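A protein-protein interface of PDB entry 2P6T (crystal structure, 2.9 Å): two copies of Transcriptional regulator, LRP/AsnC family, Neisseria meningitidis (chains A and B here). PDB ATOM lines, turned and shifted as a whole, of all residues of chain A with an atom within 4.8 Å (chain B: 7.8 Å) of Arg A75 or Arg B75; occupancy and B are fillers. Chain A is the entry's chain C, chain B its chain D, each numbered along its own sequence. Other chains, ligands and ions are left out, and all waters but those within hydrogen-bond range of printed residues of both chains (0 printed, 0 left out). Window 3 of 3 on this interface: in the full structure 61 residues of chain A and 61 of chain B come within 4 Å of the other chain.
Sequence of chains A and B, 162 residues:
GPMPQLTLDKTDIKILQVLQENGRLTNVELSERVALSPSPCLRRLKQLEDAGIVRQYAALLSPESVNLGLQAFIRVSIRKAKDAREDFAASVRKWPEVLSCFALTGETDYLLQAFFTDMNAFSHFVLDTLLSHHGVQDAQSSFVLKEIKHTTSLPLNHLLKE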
ATOM      1  N   PHE A  73      -2.839  30.236  13.227  1.00  0.00           N
ATOM      2  CA  PHE A  73      -3.887  29.497  12.529  1.00  0.00           C
ATOM      3  C   PHE A  73      -4.585  30.413  11.514  1.00  0.00           C
ATOM      4  O   PHE A  73      -5.348  31.307  11.900  1.00  0.00           O
ATOM      5  CB  PHE A  73      -4.888  28.923  13.540  1.00  0.00           C
ATOM      6  CG  PHE A  73      -4.328  27.787  14.375  1.00  0.00           C
ATOM      7  CD1 PHE A  73      -4.793  26.486  14.212  1.00  0.00           C
ATOM      8  CD2 PHE A  73      -3.326  28.016  15.314  1.00  0.00           C
ATOM      9  CE1 PHE A  73      -4.271  25.434  14.978  1.00  0.00           C
ATOM     10  CE2 PHE A  73      -2.800  26.972  16.089  1.00  0.00           C
ATOM     11  CZ  PHE A  73      -3.272  25.681  15.920  1.00  0.00           C
ATOM     12  N   ILE A  74      -4.305  30.185  10.226  1.00  0.00           N
ATOM     13  CA  ILE A  74      -4.876  30.985   9.134  1.00  0.00           C
ATOM     14  C   ILE A  74      -6.114  30.318   8.541  1.00  0.00           C
ATOM     15  O   ILE A  74      -6.018  29.218   7.997  1.00  0.00           O
ATOM     16  CB  ILE A  74      -3.883  31.173   7.961  1.00  0.00           C
ATOM     17  CG1 ILE A  74      -2.489  31.556   8.454  1.00  0.00           C
ATOM     18  CG2 ILE A  74      -4.397  32.244   6.996  1.00  0.00           C
ATOM     19  CD1 ILE A  74      -1.494  31.718   7.325  1.00  0.00           C
ATOM     20  N   ARG A  75      -7.266  30.982   8.630  1.00  0.00           N
ATOM     21  CA  ARG A  75      -8.503  30.460   8.042  1.00  0.00           C
ATOM     22  C   ARG A  75      -8.595  30.971   6.613  1.00  0.00           C
ATOM     23  O   ARG A  75      -8.977  32.120   6.374  1.00  0.00           O
ATOM     24  CB  ARG A  75      -9.751  30.877   8.836  1.00  0.00           C
ATOM     25  CG  ARG A  75      -9.628  30.808  10.368  1.00  0.00           C
ATOM     26  CD  ARG A  75     -10.805  30.085  11.042  1.00  0.00           C
ATOM     27  NE  ARG A  75     -10.449  28.712  11.408  1.00  0.00           N
ATOM     28  CZ  ARG A  75     -11.294  27.810  11.909  1.00  0.00           C
ATOM     29  NH1 ARG A  75     -12.571  28.114  12.133  1.00  0.00           N
ATOM     30  NH2 ARG A  75     -10.850  26.590  12.204  1.00  0.00           N
ATOM     31  N   VAL A  76      -8.225  30.114   5.668  1.00  0.00           N
ATOM     32  CA  VAL A  76      -8.171  30.478   4.254  1.00  0.00           C
ATOM     33  C   VAL A  76      -9.556  30.321   3.624  1.00  0.00           C
ATOM     34  O   VAL A  76     -10.440  29.687   4.207  1.00  0.00           O
ATOM     35  CB  VAL A  76      -7.153  29.591   3.503  1.00  0.00           C
ATOM     36  CG1 VAL A  76      -6.974  30.048   2.065  1.00  0.00           C
ATOM     37  CG2 VAL A  76      -5.816  29.588   4.228  1.00  0.00           C
ATOM     38  N   SER A  77      -9.745  30.940   2.458  1.00  0.00           N
ATOM     39  CA  SER A  77     -10.948  30.759   1.641  1.00  0.00           C
ATOM     40  C   SER A  77     -10.535  30.703   0.183  1.00  0.00           C
ATOM     41  O   SER A  77      -9.947  31.650  -0.333  1.00  0.00           O
ATOM     42  CB  SER A  77     -11.938  31.903   1.860  1.00  0.00           C
ATOM     43  OG  SER A  77     -12.596  31.769   3.105  1.00  0.00           O
ATOM     44  N   LEU A 104     -11.882  22.061   6.247  1.00  0.00           N
ATOM     45  CA  LEU A 104     -12.819  21.861   7.347  1.00  0.00           C
ATOM     46  C   LEU A 104     -14.218  22.227   6.955  1.00  0.00           C
ATOM     47  O   LEU A 104     -14.446  22.930   5.972  1.00  0.00           O
ATOM     48  CB  LEU A 104     -12.447  22.718   8.549  1.00  0.00           C
ATOM     49  CG  LEU A 104     -11.015  22.590   9.043  1.00  0.00           C
ATOM     50  CD1 LEU A 104     -10.757  23.599  10.149  1.00  0.00           C
ATOM     51  CD2 LEU A 104     -10.749  21.156   9.510  1.00  0.00           C
ATOM     52  N   THR A 108     -15.226  28.286   7.441  1.00  0.00           N
ATOM     53  CA  THR A 108     -13.863  28.156   6.964  1.00  0.00           C
ATOM     54  C   THR A 108     -13.749  27.064   5.907  1.00  0.00           C
ATOM     55  O   THR A 108     -14.134  25.920   6.151  1.00  0.00           O
ATOM     56  CB  THR A 108     -12.923  27.799   8.127  1.00  0.00           C
ATOM     57  OG1 THR A 108     -13.387  28.421   9.336  1.00  0.00           O
ATOM     58  CG2 THR A 108     -11.513  28.251   7.822  1.00  0.00           C
ATOM     59  N   TYR A 110     -10.604  26.275   4.282  1.00  0.00           N
ATOM     60  CA  TYR A 110      -9.348  25.619   4.673  1.00  0.00           C
ATOM     61  C   TYR A 110      -8.806  26.228   5.955  1.00  0.00           C
ATOM     62  O   TYR A 110      -9.033  27.410   6.223  1.00  0.00           O
ATOM     63  CB  TYR A 110      -8.272  25.820   3.615  1.00  0.00           C
ATOM     64  CG  TYR A 110      -8.462  25.049   2.352  1.00  0.00           C
ATOM     65  CD1 TYR A 110      -7.824  23.837   2.163  1.00  0.00           C
ATOM     66  CD2 TYR A 110      -9.254  25.547   1.332  1.00  0.00           C
ATOM     67  CE1 TYR A 110      -7.978  23.126   0.989  1.00  0.00           C
ATOM     68  CE2 TYR A 110      -9.420  24.849   0.159  1.00  0.00           C
ATOM     69  CZ  TYR A 110      -8.779  23.635  -0.014  1.00  0.00           C
ATOM     70  OH  TYR A 110      -8.936  22.930  -1.192  1.00  0.00           O
ATOM     71  N   LEU A 111      -8.057  25.434   6.718  1.00  0.00           N
ATOM     72  CA  LEU A 111      -7.375  25.930   7.910  1.00  0.00           C
ATOM     73  C   LEU A 111      -5.917  25.548   7.813  1.00  0.00           C
ATOM     74  O   LEU A 111      -5.614  24.387   7.533  1.00  0.00           O
ATOM     75  CB  LEU A 111      -7.976  25.325   9.179  1.00  0.00           C
ATOM     76  CG  LEU A 111      -7.264  25.669  10.486  1.00  0.00           C
ATOM     77  CD1 LEU A 111      -7.476  27.118  10.806  1.00  0.00           C
ATOM     78  CD2 LEU A 111      -7.771  24.792  11.602  1.00  0.00           C
ATOM     79  N   ASP A 138      -9.576  34.986   0.290  1.00  0.00           N
ATOM     80  CA  ASP A 138      -9.430  35.729   1.547  1.00  0.00           C
ATOM     81  C   ASP A 138      -8.767  34.885   2.638  1.00  0.00           C
ATOM     82  O   ASP A 138      -8.871  33.659   2.638  1.00  0.00           O
ATOM     83  CB  ASP A 138     -10.781  36.242   2.050  1.00  0.00           C
ATOM     84  CG  ASP A 138     -10.629  37.268   3.157  1.00  0.00           C
ATOM     85  OD1 ASP A 138     -10.725  38.493   2.870  1.00  0.00           O
ATOM     86  OD2 ASP A 138     -10.389  36.850   4.317  1.00  0.00           O
ATOM     87  N   ALA A 139      -8.085  35.552   3.563  1.00  0.00           N
ATOM     88  CA  ALA A 139      -7.444  34.883   4.687  1.00  0.00           C
ATOM     89  C   ALA A 139      -7.702  35.669   5.963  1.00  0.00           C
ATOM     90  O   ALA A 139      -7.611  36.895   5.966  1.00  0.00           O
ATOM     91  CB  ALA A 139      -5.956  34.760   4.444  1.00  0.00           C
ATOM     92  N   GLN A 140      -8.046  34.960   7.037  1.00  0.00           N
ATOM     93  CA  GLN A 140      -8.158  35.562   8.365  1.00  0.00           C
ATOM     94  C   GLN A 140      -7.375  34.690   9.349  1.00  0.00           C
ATOM     95  O   GLN A 140      -7.577  33.477   9.410  1.00  0.00           O
ATOM     96  CB  GLN A 140      -9.627  35.723   8.789  1.00  0.00           C
ATOM     97  CG  GLN A 140     -10.461  34.432   8.780  1.00  0.00           C
ATOM     98  CD  GLN A 140     -11.793  34.551   9.540  1.00  0.00           C
ATOM     99  OE1 GLN A 140     -11.827  34.967  10.704  1.00  0.00           O
ATOM    100  NE2 GLN A 140     -12.888  34.157   8.887  1.00  0.00           N
ATOM    101  N   SER A 141      -6.471  35.301  10.106  1.00  0.00           N
ATOM    102  CA  SER A 141      -5.516  34.541  10.910  1.00  0.00           C
ATOM    103  C   SER A 141      -5.501  34.920  12.401  1.00  0.00           C
ATOM    104  O   SER A 141      -5.500  36.093  12.749  1.00  0.00           O
ATOM    105  CB  SER A 141      -4.122  34.686  10.286  1.00  0.00           C
ATOM    106  OG  SER A 141      -4.071  35.810   9.419  1.00  0.00           O
ATOM    107  N   ALA B  72     -11.552  16.315  14.549  1.00  0.00           N
ATOM    108  CA  ALA B  72     -12.386  17.487  14.819  1.00  0.00           C
ATOM    109  C   ALA B  72     -11.585  18.631  15.422  1.00  0.00           C
ATOM    110  O   ALA B  72     -10.660  18.405  16.200  1.00  0.00           O
ATOM    111  CB  ALA B  72     -13.523  17.103  15.752  1.00  0.00           C
ATOM    112  N   PHE B  73     -11.948  19.857  15.054  1.00  0.00           N
ATOM    113  CA  PHE B  73     -11.411  21.055  15.689  1.00  0.00           C
ATOM    114  C   PHE B  73     -12.540  21.733  16.454  1.00  0.00           C
ATOM    115  O   PHE B  73     -13.579  22.027  15.871  1.00  0.00           O
ATOM    116  CB  PHE B  73     -10.826  22.005  14.648  1.00  0.00           C
ATOM    117  CG  PHE B  73      -9.513  21.555  14.085  1.00  0.00           C
ATOM    118  CD1 PHE B  73      -8.404  21.403  14.908  1.00  0.00           C
ATOM    119  CD2 PHE B  73      -9.375  21.298  12.722  1.00  0.00           C
ATOM    120  CE1 PHE B  73      -7.176  20.990  14.379  1.00  0.00           C
ATOM    121  CE2 PHE B  73      -8.152  20.886  12.179  1.00  0.00           C
ATOM    122  CZ  PHE B  73      -7.050  20.733  13.006  1.00  0.00           C
ATOM    123  N   ILE B  74     -12.352  21.957  17.754  1.00  0.00           N
ATOM    124  CA  ILE B  74     -13.400  22.560  18.589  1.00  0.00           C
ATOM    125  C   ILE B  74     -12.994  23.925  19.127  1.00  0.00           C
ATOM    126  O   ILE B  74     -11.966  24.068  19.802  1.00  0.00           O
ATOM    127  CB  ILE B  74     -13.789  21.698  19.815  1.00  0.00           C
ATOM    128  CG1 ILE B  74     -13.976  20.232  19.438  1.00  0.00           C
ATOM    129  CG2 ILE B  74     -15.080  22.215  20.432  1.00  0.00           C
ATOM    130  CD1 ILE B  74     -14.463  19.381  20.602  1.00  0.00           C
ATOM    131  N   ARG B  75     -13.835  24.918  18.842  1.00  0.00           N
ATOM    132  CA  ARG B  75     -13.656  26.269  19.348  1.00  0.00           C
ATOM    133  C   ARG B  75     -14.457  26.392  20.652  1.00  0.00           C
ATOM    134  O   ARG B  75     -15.687  26.486  20.640  1.00  0.00           O
ATOM    135  CB  ARG B  75     -14.082  27.300  18.285  1.00  0.00           C
ATOM    136  CG  ARG B  75     -13.451  27.033  16.893  1.00  0.00           C
ATOM    137  CD  ARG B  75     -13.692  28.142  15.850  1.00  0.00           C
ATOM    138  NE  ARG B  75     -12.631  29.159  15.825  1.00  0.00           N
ATOM    139  CZ  ARG B  75     -11.400  28.983  15.331  1.00  0.00           C
ATOM    140  NH1 ARG B  75     -11.030  27.813  14.819  1.00  0.00           N
ATOM    141  NH2 ARG B  75     -10.521  29.984  15.365  1.00  0.00           N
ATOM    142  N   VAL B  76     -13.735  26.340  21.770  1.00  0.00           N
ATOM    143  CA  VAL B  76     -14.311  26.419  23.111  1.00  0.00           C
ATOM    144  C   VAL B  76     -14.178  27.830  23.671  1.00  0.00           C
ATOM    145  O   VAL B  76     -13.263  28.566  23.299  1.00  0.00           O
ATOM    146  CB  VAL B  76     -13.594  25.444  24.071  1.00  0.00           C
ATOM    147  CG1 VAL B  76     -13.982  25.710  25.533  1.00  0.00           C
ATOM    148  CG2 VAL B  76     -13.897  24.018  23.676  1.00  0.00           C
ATOM    149  N   SER B  77     -15.093  28.194  24.567  1.00  0.00           N
ATOM    150  CA  SER B  77     -15.050  29.480  25.257  1.00  0.00           C
ATOM    151  C   SER B  77     -15.143  29.262  26.757  1.00  0.00           C
ATOM    152  O   SER B  77     -16.099  28.658  27.251  1.00  0.00           O
ATOM    153  CB  SER B  77     -16.201  30.367  24.803  1.00  0.00           C
ATOM    154  OG  SER B  77     -17.440  29.700  24.983  1.00  0.00           O
ATOM    155  N   ILE B  78     -14.150  29.763  27.480  1.00  0.00           N
ATOM    156  CA  ILE B  78     -14.107  29.596  28.919  1.00  0.00           C
ATOM    157  C   ILE B  78     -15.117  30.521  29.569  1.00  0.00           C
ATOM    158  O   ILE B  78     -15.483  31.546  28.996  1.00  0.00           O
ATOM    159  CB  ILE B  78     -12.715  29.937  29.464  1.00  0.00           C
ATOM    160  CG1 ILE B  78     -12.367  29.033  30.641  1.00  0.00           C
ATOM    161  CG2 ILE B  78     -12.622  31.421  29.839  1.00  0.00           C
ATOM    162  CD1 ILE B  78     -11.979  27.626  30.218  1.00  0.00           C
ATOM    163  N   LEU B 104      -6.092  30.872  21.649  1.00  0.00           N
ATOM    164  CA  LEU B 104      -5.905  31.699  20.472  1.00  0.00           C
ATOM    165  C   LEU B 104      -6.399  33.099  20.715  1.00  0.00           C
ATOM    166  O   LEU B 104      -7.110  33.369  21.675  1.00  0.00           O
ATOM    167  CB  LEU B 104      -6.647  31.112  19.259  1.00  0.00           C
ATOM    168  CG  LEU B 104      -5.995  29.899  18.573  1.00  0.00           C
ATOM    169  CD1 LEU B 104      -6.831  29.413  17.382  1.00  0.00           C
ATOM    170  CD2 LEU B 104      -4.572  30.244  18.122  1.00  0.00           C
ATOM    171  N   THR B 105      -6.012  33.988  19.815  1.00  0.00           N
ATOM    172  CA  THR B 105      -6.580  35.309  19.762  1.00  0.00           C
ATOM    173  C   THR B 105      -7.866  35.178  18.955  1.00  0.00           C
ATOM    174  O   THR B 105      -8.168  34.104  18.435  1.00  0.00           O
ATOM    175  CB  THR B 105      -5.606  36.263  19.100  1.00  0.00           C
ATOM    176  OG1 THR B 105      -5.466  35.911  17.720  1.00  0.00           O
ATOM    177  CG2 THR B 105      -4.253  36.168  19.784  1.00  0.00           C
ATOM    178  N   GLY B 106      -8.637  36.253  18.873  1.00  0.00           N
ATOM    179  CA  GLY B 106      -9.862  36.256  18.069  1.00  0.00           C
ATOM    180  C   GLY B 106     -11.115  35.934  18.861  1.00  0.00           C
ATOM    181  O   GLY B 106     -11.091  35.893  20.095  1.00  0.00           O
ATOM    182  N   GLU B 107     -12.216  35.699  18.155  1.00  0.00           N
ATOM    183  CA  GLU B 107     -13.489  35.411  18.816  1.00  0.00           C
ATOM    184  C   GLU B 107     -13.453  34.121  19.620  1.00  0.00           C
ATOM    185  O   GLU B 107     -14.207  33.970  20.582  1.00  0.00           O
ATOM    186  CB  GLU B 107     -14.647  35.363  17.815  1.00  0.00           C
ATOM    187  CG  GLU B 107     -15.651  36.492  18.002  1.00  0.00           C
ATOM    188  CD  GLU B 107     -16.797  36.430  17.015  1.00  0.00           C
ATOM    189  OE1 GLU B 107     -17.263  35.311  16.703  1.00  0.00           O
ATOM    190  OE2 GLU B 107     -17.242  37.504  16.557  1.00  0.00           O
ATOM    191  N   THR B 108     -12.579  33.201  19.222  1.00  0.00           N
ATOM    192  CA  THR B 108     -12.390  31.939  19.937  1.00  0.00           C
ATOM    193  C   THR B 108     -11.424  32.135  21.115  1.00  0.00           C
ATOM    194  O   THR B 108     -10.370  32.759  20.960  1.00  0.00           O
ATOM    195  CB  THR B 108     -11.881  30.820  18.972  1.00  0.00           C
ATOM    196  OG1 THR B 108     -11.871  29.557  19.648  1.00  0.00           O
ATOM    197  CG2 THR B 108     -10.476  31.135  18.423  1.00  0.00           C
ATOM    198  N   ASP B 109     -11.798  31.635  22.291  1.00  0.00           N
ATOM    199  CA  ASP B 109     -10.912  31.685  23.463  1.00  0.00           C
ATOM    200  C   ASP B 109      -9.922  30.517  23.442  1.00  0.00           C
ATOM    201  O   ASP B 109      -8.742  30.707  23.715  1.00  0.00           O
ATOM    202  CB  ASP B 109     -11.711  31.671  24.779  1.00  0.00           C
ATOM    203  CG  ASP B 109     -12.493  32.961  25.013  1.00  0.00           C
ATOM    204  OD1 ASP B 109     -11.887  34.052  24.996  1.00  0.00           O
ATOM    205  OD2 ASP B 109     -13.718  32.883  25.236  1.00  0.00           O
ATOM    206  N   TYR B 110     -10.417  29.318  23.122  1.00  0.00           N
ATOM    207  CA  TYR B 110      -9.598  28.109  23.050  1.00  0.00           C
ATOM    208  C   TYR B 110      -9.905  27.286  21.821  1.00  0.00           C
ATOM    209  O   TYR B 110     -11.064  27.164  21.419  1.00  0.00           O
ATOM    210  CB  TYR B 110      -9.869  27.229  24.241  1.00  0.00           C
ATOM    211  CG  TYR B 110      -9.292  27.766  25.502  1.00  0.00           C
ATOM    212  CD1 TYR B 110      -7.926  27.666  25.748  1.00  0.00           C
ATOM    213  CD2 TYR B 110     -10.106  28.372  26.465  1.00  0.00           C
ATOM    214  CE1 TYR B 110      -7.380  28.148  26.918  1.00  0.00           C
ATOM    215  CE2 TYR B 110      -9.571  28.857  27.639  1.00  0.00           C
ATOM    216  CZ  TYR B 110      -8.208  28.742  27.862  1.00  0.00           C
ATOM    217  OH  TYR B 110      -7.661  29.219  29.028  1.00  0.00           O
ATOM    218  N   LEU B 111      -8.870  26.690  21.246  1.00  0.00           N
ATOM    219  CA  LEU B 111      -9.042  25.831  20.093  1.00  0.00           C
ATOM    220  C   LEU B 111      -8.520  24.457  20.461  1.00  0.00           C
ATOM    221  O   LEU B 111      -7.428  24.343  21.006  1.00  0.00           O
ATOM    222  CB  LEU B 111      -8.267  26.398  18.907  1.00  0.00           C
ATOM    223  CG  LEU B 111      -8.427  25.676  17.571  1.00  0.00           C
ATOM    224  CD1 LEU B 111      -9.745  26.026  16.900  1.00  0.00           C
ATOM    225  CD2 LEU B 111      -7.259  26.023  16.697  1.00  0.00           C
ATOM    226  N   LEU B 112      -9.306  23.420  20.180  1.00  0.00           N
ATOM    227  CA  LEU B 112      -8.935  22.044  20.508  1.00  0.00           C
ATOM    228  C   LEU B 112      -8.908  21.186  19.249  1.00  0.00           C
ATOM    229  O   LEU B 112      -9.846  21.197  18.461  1.00  0.00           O
ATOM    230  CB  LEU B 112      -9.934  21.443  21.504  1.00  0.00           C
ATOM    231  CG  LEU B 112     -10.011  22.086  22.886  1.00  0.00           C
ATOM    232  CD1 LEU B 112     -10.219  23.600  22.830  1.00  0.00           C
ATOM    233  CD2 LEU B 112     -11.125  21.446  23.699  1.00  0.00           C
ATOM    234  N   GLN B 113      -7.833  20.438  19.071  1.00  0.00           N
ATOM    235  CA  GLN B 113      -7.782  19.405  18.050  1.00  0.00           C
ATOM    236  C   GLN B 113      -8.073  18.088  18.759  1.00  0.00           C
ATOM    237  O   GLN B 113      -7.509  17.817  19.821  1.00  0.00           O
ATOM    238  CB  GLN B 113      -6.406  19.378  17.383  1.00  0.00           C
ATOM    239  CG  GLN B 113      -6.247  18.362  16.272  1.00  0.00           C
ATOM    240  CD  GLN B 113      -4.924  18.526  15.545  1.00  0.00           C
ATOM    241  OE1 GLN B 113      -3.871  18.649  16.174  1.00  0.00           O
ATOM    242  NE2 GLN B 113      -4.971  18.539  14.215  1.00  0.00           N
ATOM    243  N   LEU B 130     -17.186  17.543  27.596  1.00  0.00           N
ATOM    244  CA  LEU B 130     -16.749  18.903  27.318  1.00  0.00           C
ATOM    245  C   LEU B 130     -17.714  19.900  27.935  1.00  0.00           C
ATOM    246  O   LEU B 130     -17.320  20.720  28.755  1.00  0.00           O
ATOM    247  CB  LEU B 130     -16.624  19.135  25.806  1.00  0.00           C
ATOM    248  CG  LEU B 130     -16.119  20.516  25.374  1.00  0.00           C
ATOM    249  CD1 LEU B 130     -14.703  20.757  25.871  1.00  0.00           C
ATOM    250  CD2 LEU B 130     -16.186  20.665  23.863  1.00  0.00           C
ATOM    251  N   VAL B 136     -16.625  25.319  30.929  1.00  0.00           N
ATOM    252  CA  VAL B 136     -16.948  25.410  29.507  1.00  0.00           C
ATOM    253  C   VAL B 136     -18.283  26.102  29.296  1.00  0.00           C
ATOM    254  O   VAL B 136     -19.329  25.544  29.604  1.00  0.00           O
ATOM    255  CB  VAL B 136     -17.004  24.035  28.842  1.00  0.00           C
ATOM    256  CG1 VAL B 136     -17.233  24.190  27.345  1.00  0.00           C
ATOM    257  CG2 VAL B 136     -15.723  23.283  29.098  1.00  0.00           C
ATOM    258  N   ASP B 138     -19.406  27.530  26.197  1.00  0.00           N
ATOM    259  CA  ASP B 138     -19.975  27.135  24.907  1.00  0.00           C
ATOM    260  C   ASP B 138     -18.894  26.464  24.075  1.00  0.00           C
ATOM    261  O   ASP B 138     -17.728  26.844  24.153  1.00  0.00           O
ATOM    262  CB  ASP B 138     -20.526  28.354  24.146  1.00  0.00           C
ATOM    263  CG  ASP B 138     -21.242  27.972  22.834  1.00  0.00           C
ATOM    264  OD1 ASP B 138     -22.465  27.697  22.873  1.00  0.00           O
ATOM    265  OD2 ASP B 138     -20.592  27.969  21.759  1.00  0.00           O
ATOM    266  N   ALA B 139     -19.291  25.470  23.286  1.00  0.00           N
ATOM    267  CA  ALA B 139     -18.392  24.807  22.338  1.00  0.00           C
ATOM    268  C   ALA B 139     -18.935  24.921  20.925  1.00  0.00           C
ATOM    269  O   ALA B 139     -20.140  25.050  20.722  1.00  0.00           O
ATOM    270  CB  ALA B 139     -18.205  23.347  22.708  1.00  0.00           C
ATOM    271  N   GLN B 140     -18.039  24.861  19.949  1.00  0.00           N
ATOM    272  CA  GLN B 140     -18.415  25.074  18.557  1.00  0.00           C
ATOM    273  C   GLN B 140     -17.420  24.358  17.651  1.00  0.00           C
ATOM    274  O   GLN B 140     -16.284  24.810  17.485  1.00  0.00           O
ATOM    275  CB  GLN B 140     -18.428  26.578  18.300  1.00  0.00           C
ATOM    276  CG  GLN B 140     -18.719  27.035  16.887  1.00  0.00           C
ATOM    277  CD  GLN B 140     -18.381  28.499  16.731  1.00  0.00           C
ATOM    278  OE1 GLN B 140     -17.231  28.900  16.922  1.00  0.00           O
ATOM    279  NE2 GLN B 140     -19.383  29.316  16.413  1.00  0.00           N
ATOM    280  N   SER B 141     -17.839  23.245  17.057  1.00  0.00           N
ATOM    281  CA  SER B 141     -16.888  22.356  16.385  1.00  0.00           C
ATOM    282  C   SER B 141     -17.091  22.153  14.886  1.00  0.00           C
ATOM    283  O   SER B 141     -18.204  21.996  14.391  1.00  0.00           O
ATOM    284  CB  SER B 141     -16.871  21.002  17.087  1.00  0.00           C
ATOM    285  OG  SER B 141     -18.193  20.572  17.361  1.00  0.00           O
ATOM    286  N   SER B 142     -15.967  22.153  14.180  1.00  0.00           N
ATOM    287  CA  SER B 142     -15.916  21.835  12.762  1.00  0.00           C
ATOM    288  C   SER B 142     -15.075  20.589  12.577  1.00  0.00           C
ATOM    289  O   SER B 142     -14.214  20.293  13.399  1.00  0.00           O
ATOM    290  CB  SER B 142     -15.285  22.981  11.988  1.00  0.00           C
ATOM    291  OG  SER B 142     -14.819  22.537  10.729  1.00  0.00           O
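The guanidinium group (NH2) of Arg A75 sits close to the guanidinium group (NH1) of Arg B75 (2.9 Å).
O of Gln A140 sits at hydrogen-bond distance from N of Arg A75 (2.6 Å). The backbone NH (N) of Leu B104 sits at hydrogen-bond distance from the backbone carbonyl oxygen (O) of Asp B109. O of Gln B140 lies within hydrogen-bond range of N of Arg B75. The guanidinium group of Arg A75 sits at hydrogen-bond distance from the side-chain hydroxyl of Thr A108, at 2.9 Å. N of Phe B73 lies within hydrogen-bond range of O of Ser B142, 2.8 Å away.
Printed residues of chain B within 4 Å of Arg A75: Arg B75 (2.9 Å). Of the printed residues of chain A, Arg B75 touches Arg A75 (2.9 Å). Of the printed residues of chain A, Ser B142 touches Leu A104 (3.2 Å). Printed residues of chain B within 4 Å of Phe A73: Leu B104 (3.8 Å) and Leu B111 (3.5 Å). Printed residues of chain A within 4 Å of Leu B104: Phe A73 (3.8 Å). Of the printed residues of chain B, Leu A104 touches Phe B73 (3.5 Å) and Ser B142 (3.2 Å). Ala A139 touches none of the printed residues of chain B. Ser A77 touches none of the printed residues of chain B. The nearest residue of chain B that does not touch Arg A75 is Leu B111 (4.9 Å).
Printed residues of chain A that touch a printed residue of chain B: Phe A73, Arg A75, Leu A104 and Leu A111. Hydrophobic or aromatic side chains of chain A that line the printed part of chain B: Phe A73, Leu A104 and Leu A111. Among the printed residues, 6 pairs touch across the chains. Among the printed residues, no Asp or Glu carboxylate lies within 4 Å of a Lys or Arg side-chain nitrogen of the other chain.
Among the printed residues, merely in contact across the chains: Phe A73 with Leu B104, Phe A73 with Leu B111, Leu A104 with Phe B73, Leu A104 with Ser B142 and Leu A111 with Phe B73.
Phe A73 touches Leu B104, and with the chains exchanged Leu A104 touches Phe B73. Phe A73 touches Leu B111, and with the chains exchanged Leu A111 touches Phe B73. Arg A75 touches its own counterpart, Arg B75. Of the 6 pairs that touch across the chains among the printed residues, 5 have their exchanged pair printed and touching as well.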
